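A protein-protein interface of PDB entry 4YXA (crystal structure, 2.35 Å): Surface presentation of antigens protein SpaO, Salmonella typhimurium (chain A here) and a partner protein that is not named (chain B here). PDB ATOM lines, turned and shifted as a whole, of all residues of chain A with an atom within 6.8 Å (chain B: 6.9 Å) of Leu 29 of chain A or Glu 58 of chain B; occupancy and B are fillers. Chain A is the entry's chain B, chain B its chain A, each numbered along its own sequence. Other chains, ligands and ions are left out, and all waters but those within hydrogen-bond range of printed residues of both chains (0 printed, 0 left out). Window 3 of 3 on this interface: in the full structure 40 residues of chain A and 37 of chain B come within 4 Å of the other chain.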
ATOM      1  N   ALA A  23      14.050  15.988   4.997  1.00  0.00           N
ATOM      2  CA  ALA A  23      13.583  14.851   4.209  1.00  0.00           C
ATOM      3  C   ALA A  23      14.593  13.714   4.179  1.00  0.00           C
ATOM      4  O   ALA A  23      14.334  12.673   3.582  1.00  0.00           O
ATOM      5  CB  ALA A  23      13.251  15.289   2.779  1.00  0.00           C
ATOM      6  N   MET A  24      15.744  13.920   4.807  1.00  0.00           N
ATOM      7  CA  MET A  24      16.783  12.907   4.846  1.00  0.00           C
ATOM      8  C   MET A  24      17.214  12.635   6.278  1.00  0.00           C
ATOM      9  O   MET A  24      17.748  11.575   6.586  1.00  0.00           O
ATOM     10  CB  MET A  24      17.966  13.343   4.004  1.00  0.00           C
ATOM     11  CG  MET A  24      19.144  12.420   4.055  1.00  0.00           C
ATOM     12  SD  MET A  24      20.530  13.234   2.995  1.00  0.00           S
ATOM     13  CE  MET A  24      20.896  14.765   4.157  1.00  0.00           C
ATOM     14  N   GLN A  27      16.032   9.192   7.045  1.00  0.00           N
ATOM     15  CA  GLN A  27      16.601   8.010   6.387  1.00  0.00           C
ATOM     16  C   GLN A  27      16.045   7.797   4.987  1.00  0.00           C
ATOM     17  O   GLN A  27      15.573   6.707   4.653  1.00  0.00           O
ATOM     18  CB  GLN A  27      16.380   6.734   7.213  1.00  0.00           C
ATOM     19  CG  GLN A  27      16.407   6.831   8.763  1.00  0.00           C
ATOM     20  CD  GLN A  27      17.174   8.010   9.363  1.00  0.00           C
ATOM     21  OE1 GLN A  27      18.123   8.522   8.781  1.00  0.00           O
ATOM     22  NE2 GLN A  27      16.764   8.424  10.555  1.00  0.00           N
ATOM     23  N   GLN A  28      16.107   8.842   4.168  1.00  0.00           N
ATOM     24  CA  GLN A  28      15.804   8.708   2.755  1.00  0.00           C
ATOM     25  C   GLN A  28      17.067   8.341   2.001  1.00  0.00           C
ATOM     26  O   GLN A  28      18.143   8.869   2.286  1.00  0.00           O
ATOM     27  CB  GLN A  28      15.231   9.996   2.186  1.00  0.00           C
ATOM     28  CG  GLN A  28      14.890   9.905   0.705  1.00  0.00           C
ATOM     29  CD  GLN A  28      14.727  11.268   0.055  1.00  0.00           C
ATOM     30  OE1 GLN A  28      15.304  12.256   0.512  1.00  0.00           O
ATOM     31  NE2 GLN A  28      13.940  11.327  -1.011  1.00  0.00           N
ATOM     32  N   LEU A  29      16.929   7.438   1.040  1.00  0.00           N
ATOM     33  CA  LEU A  29      18.049   7.037   0.210  1.00  0.00           C
ATOM     34  C   LEU A  29      18.508   8.171  -0.678  1.00  0.00           C
ATOM     35  O   LEU A  29      17.788   8.595  -1.578  1.00  0.00           O
ATOM     36  CB  LEU A  29      17.679   5.844  -0.667  1.00  0.00           C
ATOM     37  CG  LEU A  29      18.800   5.396  -1.609  1.00  0.00           C
ATOM     38  CD1 LEU A  29      19.971   4.812  -0.819  1.00  0.00           C
ATOM     39  CD2 LEU A  29      18.306   4.430  -2.673  1.00  0.00           C
ATOM     40  N   LEU A  30      19.715   8.653  -0.432  1.00  0.00           N
ATOM     41  CA  LEU A  30      20.325   9.602  -1.340  1.00  0.00           C
ATOM     42  C   LEU A  30      21.045   8.840  -2.455  1.00  0.00           C
ATOM     43  O   LEU A  30      22.022   8.135  -2.221  1.00  0.00           O
ATOM     44  CB  LEU A  30      21.277  10.532  -0.591  1.00  0.00           C
ATOM     45  CG  LEU A  30      21.817  11.679  -1.444  1.00  0.00           C
ATOM     46  CD1 LEU A  30      21.818  12.970  -0.662  1.00  0.00           C
ATOM     47  CD2 LEU A  30      23.211  11.350  -1.891  1.00  0.00           C
ATOM     48  N   SER A  31      20.545   8.984  -3.674  1.00  0.00           N
ATOM     49  CA  SER A  31      21.050   8.209  -4.801  1.00  0.00           C
ATOM     50  C   SER A  31      22.460   8.598  -5.209  1.00  0.00           C
ATOM     51  O   SER A  31      22.737   9.751  -5.541  1.00  0.00           O
ATOM     52  CB  SER A  31      20.127   8.349  -6.021  1.00  0.00           C
ATOM     53  OG  SER A  31      18.783   8.029  -5.713  1.00  0.00           O
ATOM     54  N   LEU A  32      23.334   7.602  -5.211  1.00  0.00           N
ATOM     55  CA  LEU A  32      24.655   7.726  -5.798  1.00  0.00           C
ATOM     56  C   LEU A  32      24.788   6.824  -7.021  1.00  0.00           C
ATOM     57  O   LEU A  32      24.072   5.831  -7.150  1.00  0.00           O
ATOM     58  CB  LEU A  32      25.732   7.360  -4.780  1.00  0.00           C
ATOM     59  CG  LEU A  32      25.692   8.067  -3.438  1.00  0.00           C
ATOM     60  CD1 LEU A  32      26.875   7.640  -2.624  1.00  0.00           C
ATOM     61  CD2 LEU A  32      25.746   9.535  -3.676  1.00  0.00           C
ATOM     62  N   ASN B  55      25.815   6.180   6.348  1.00  0.00           N
ATOM     63  CA  ASN B  55      26.559   4.994   5.971  1.00  0.00           C
ATOM     64  C   ASN B  55      26.229   4.555   4.570  1.00  0.00           C
ATOM     65  O   ASN B  55      25.142   4.809   4.065  1.00  0.00           O
ATOM     66  CB  ASN B  55      26.319   3.851   6.957  1.00  0.00           C
ATOM     67  CG  ASN B  55      27.548   3.559   7.823  1.00  0.00           C
ATOM     68  OD1 ASN B  55      28.687   3.785   7.404  1.00  0.00           O
ATOM     69  ND2 ASN B  55      27.319   3.047   9.029  1.00  0.00           N
ATOM     70  N   ARG B  56      27.201   3.893   3.957  1.00  0.00           N
ATOM     71  CA  ARG B  56      27.165   3.522   2.557  1.00  0.00           C
ATOM     72  C   ARG B  56      26.304   2.298   2.347  1.00  0.00           C
ATOM     73  O   ARG B  56      26.643   1.221   2.819  1.00  0.00           O
ATOM     74  CB  ARG B  56      28.585   3.259   2.070  1.00  0.00           C
ATOM     75  CG  ARG B  56      28.707   2.931   0.612  1.00  0.00           C
ATOM     76  CD  ARG B  56      28.249   4.074  -0.261  1.00  0.00           C
ATOM     77  NE  ARG B  56      28.591   3.820  -1.650  1.00  0.00           N
ATOM     78  CZ  ARG B  56      27.751   3.994  -2.661  1.00  0.00           C
ATOM     79  NH1 ARG B  56      26.519   4.430  -2.430  1.00  0.00           N
ATOM     80  NH2 ARG B  56      28.142   3.731  -3.898  1.00  0.00           N
ATOM     81  N   VAL B  57      25.190   2.453   1.644  1.00  0.00           N
ATOM     82  CA  VAL B  57      24.240   1.358   1.508  1.00  0.00           C
ATOM     83  C   VAL B  57      23.758   1.170   0.098  1.00  0.00           C
ATOM     84  O   VAL B  57      24.094   1.958  -0.786  1.00  0.00           O
ATOM     85  CB  VAL B  57      22.988   1.572   2.370  1.00  0.00           C
ATOM     86  CG1 VAL B  57      23.353   1.887   3.806  1.00  0.00           C
ATOM     87  CG2 VAL B  57      22.153   2.691   1.786  1.00  0.00           C
ATOM     88  N   GLU B  58      22.963   0.113  -0.080  1.00  0.00           N
ATOM     89  CA  GLU B  58      22.167  -0.132  -1.279  1.00  0.00           C
ATOM     90  C   GLU B  58      22.817   0.334  -2.556  1.00  0.00           C
ATOM     91  O   GLU B  58      23.740  -0.295  -3.064  1.00  0.00           O
ATOM     92  CB  GLU B  58      20.815   0.556  -1.147  1.00  0.00           C
ATOM     93  CG  GLU B  58      19.668  -0.389  -0.897  1.00  0.00           C
ATOM     94  CD  GLU B  58      18.362   0.200  -1.362  1.00  0.00           C
ATOM     95  OE1 GLU B  58      18.347   0.773  -2.475  1.00  0.00           O
ATOM     96  OE2 GLU B  58      17.359   0.097  -0.621  1.00  0.00           O
ATOM     97  N   GLY B  59      22.299   1.448  -3.059  1.00  0.00           N
ATOM     98  CA  GLY B  59      22.854   2.159  -4.196  1.00  0.00           C
ATOM     99  C   GLY B  59      22.773   3.638  -3.871  1.00  0.00           C
ATOM    100  O   GLY B  59      22.192   4.441  -4.609  1.00  0.00           O
ATOM    101  N   GLY B  60      23.344   3.982  -2.723  1.00  0.00           N
ATOM    102  CA  GLY B  60      23.309   5.336  -2.225  1.00  0.00           C
ATOM    103  C   GLY B  60      23.745   5.402  -0.777  1.00  0.00           C
ATOM    104  O   GLY B  60      24.617   4.657  -0.334  1.00  0.00           O
ATOM    105  N   ILE B  61      23.108   6.297  -0.037  1.00  0.00           N
ATOM    106  CA  ILE B  61      23.523   6.630   1.315  1.00  0.00           C
ATOM    107  C   ILE B  61      22.301   6.886   2.176  1.00  0.00           C
ATOM    108  O   ILE B  61      21.277   7.346   1.677  1.00  0.00           O
ATOM    109  CB  ILE B  61      24.429   7.875   1.315  1.00  0.00           C
ATOM    110  CG1 ILE B  61      25.872   7.480   1.025  1.00  0.00           C
ATOM    111  CG2 ILE B  61      24.345   8.638   2.626  1.00  0.00           C
ATOM    112  CD1 ILE B  61      26.743   8.646   0.720  1.00  0.00           C
ATOM    113  N   ILE B  62      22.401   6.564   3.462  1.00  0.00           N
ATOM    114  CA  ILE B  62      21.378   6.938   4.422  1.00  0.00           C
ATOM    115  C   ILE B  62      22.024   7.646   5.597  1.00  0.00           C
ATOM    116  O   ILE B  62      22.987   7.139   6.175  1.00  0.00           O
ATOM    117  CB  ILE B  62      20.601   5.717   4.908  1.00  0.00           C
ATOM    118  CG1 ILE B  62      19.788   5.135   3.752  1.00  0.00           C
ATOM    119  CG2 ILE B  62      19.696   6.086   6.071  1.00  0.00           C
ATOM    120  CD1 ILE B  62      19.212   3.772   4.044  1.00  0.00           C
ATOM    121  N   VAL B  63      21.488   8.816   5.942  1.00  0.00           N
ATOM    122  CA  VAL B  63      22.066   9.673   6.980  1.00  0.00           C
ATOM    123  C   VAL B  63      21.346   9.563   8.311  1.00  0.00           C
ATOM    124  O   VAL B  63      20.184   9.933   8.412  1.00  0.00           O
ATOM    125  CB  VAL B  63      22.028  11.134   6.568  1.00  0.00           C
ATOM    126  CG1 VAL B  63      22.653  11.991   7.644  1.00  0.00           C
ATOM    127  CG2 VAL B  63      22.727  11.306   5.259  1.00  0.00           C
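Printed residues of chain A that touch a printed residue of chain B: Met 24, Gln 27, Gln 28, Leu 29, Leu 30, Ser 31 and Leu 32. Hydrophobic or aromatic side chains of chain A within 4 Å of the printed part of chain B: Met 24, Leu 29, Leu 30 and Leu 32. Along chain A the printed residues that touch a printed residue of chain B span positions 24 to 32. Hydrophobic or aromatic side chains of chain B within 4 Å of the printed part of chain A: Ile 61, Ile 62 and Val 63. Among the printed residues, no Asp or Glu carboxylate lies within 4 Å of a Lys or Arg side-chain nitrogen of the other chain.
N of Asn 55 of chain B is in hydrogen-bond range of O of Ile 62 of chain B, at 3.0 Å. O of Ala 23 of chain A sits close to OE1 of Gln 28 of chain A (3.2 Å). The backbone carbonyl oxygen of Gly 60 of chain B sits at hydrogen-bond distance from the guanidinium group of Arg 56 of chain B (2.8 Å).
Of the printed residues of chain B, Leu 29 of chain A touches Glu 58 (3.7 Å), Gly 60 (3.7 Å) and Ile 61 (3.6 Å). Glu 58 of chain B touches one residue of chain A. Of the printed residues of chain B, Gln 28 of chain A touches Ile 61 (3.5 Å). Of the printed residues of chain A, Ile 61 of chain B touches Gln 28 (3.5 Å), Leu 29 (3.6 Å), Leu 30 (2.9 Å) and Leu 32 (3.5 Å). Of the printed residues of chain A, Val 63 of chain B touches Met 24 (3.5 Å) and Gln 27 (2.5 Å). The nearest printed residue of chain A that does not touch Gly 59 of chain B is Leu 29 of chain A (4.3 Å).
O of Val 63 of chain B sits close to OE1 of Gln 27 of chain A, at 2.5 Å. The backbone NH (N) of Leu 32 of chain A is in hydrogen-bond range of the backbone carbonyl oxygen (O) of Gly 59 of chain B (3.4 Å). O of Val 63 of chain B sits close to O of Met 24 of chain A, 3.5 Å away. The backbone carbonyl oxygen (O) of Ile 61 of chain B lies within hydrogen-bond range of the backbone NH (N) of Leu 30 of chain A (2.9 Å).
Among the printed residues, merely in contact across the chains: Gln 27 of chain A with Ile 62 of chain B (3.6 Å), Gln 28 of chain A with Ile 61 of chain B (3.5 Å), Leu 29 of chain A with Glu 58 of chain B (3.7 Å), Leu 29 of chain A with Gly 60 of chain B (3.7 Å), Leu 29 of chain A with Ile 61 of chain B (3.6 Å), Leu 30 of chain A with Gly 60 of chain B (3.1 Å), Ser 31 of chain A with Gly 59 of chain B (3.9 Å), Leu 32 of chain A with Arg 56 of chain B (3.2 Å), Leu 32 of chain A with Gly 60 of chain B (3.7 Å) and Leu 32 of chain A with Ile 61 of chain B (3.5 Å).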
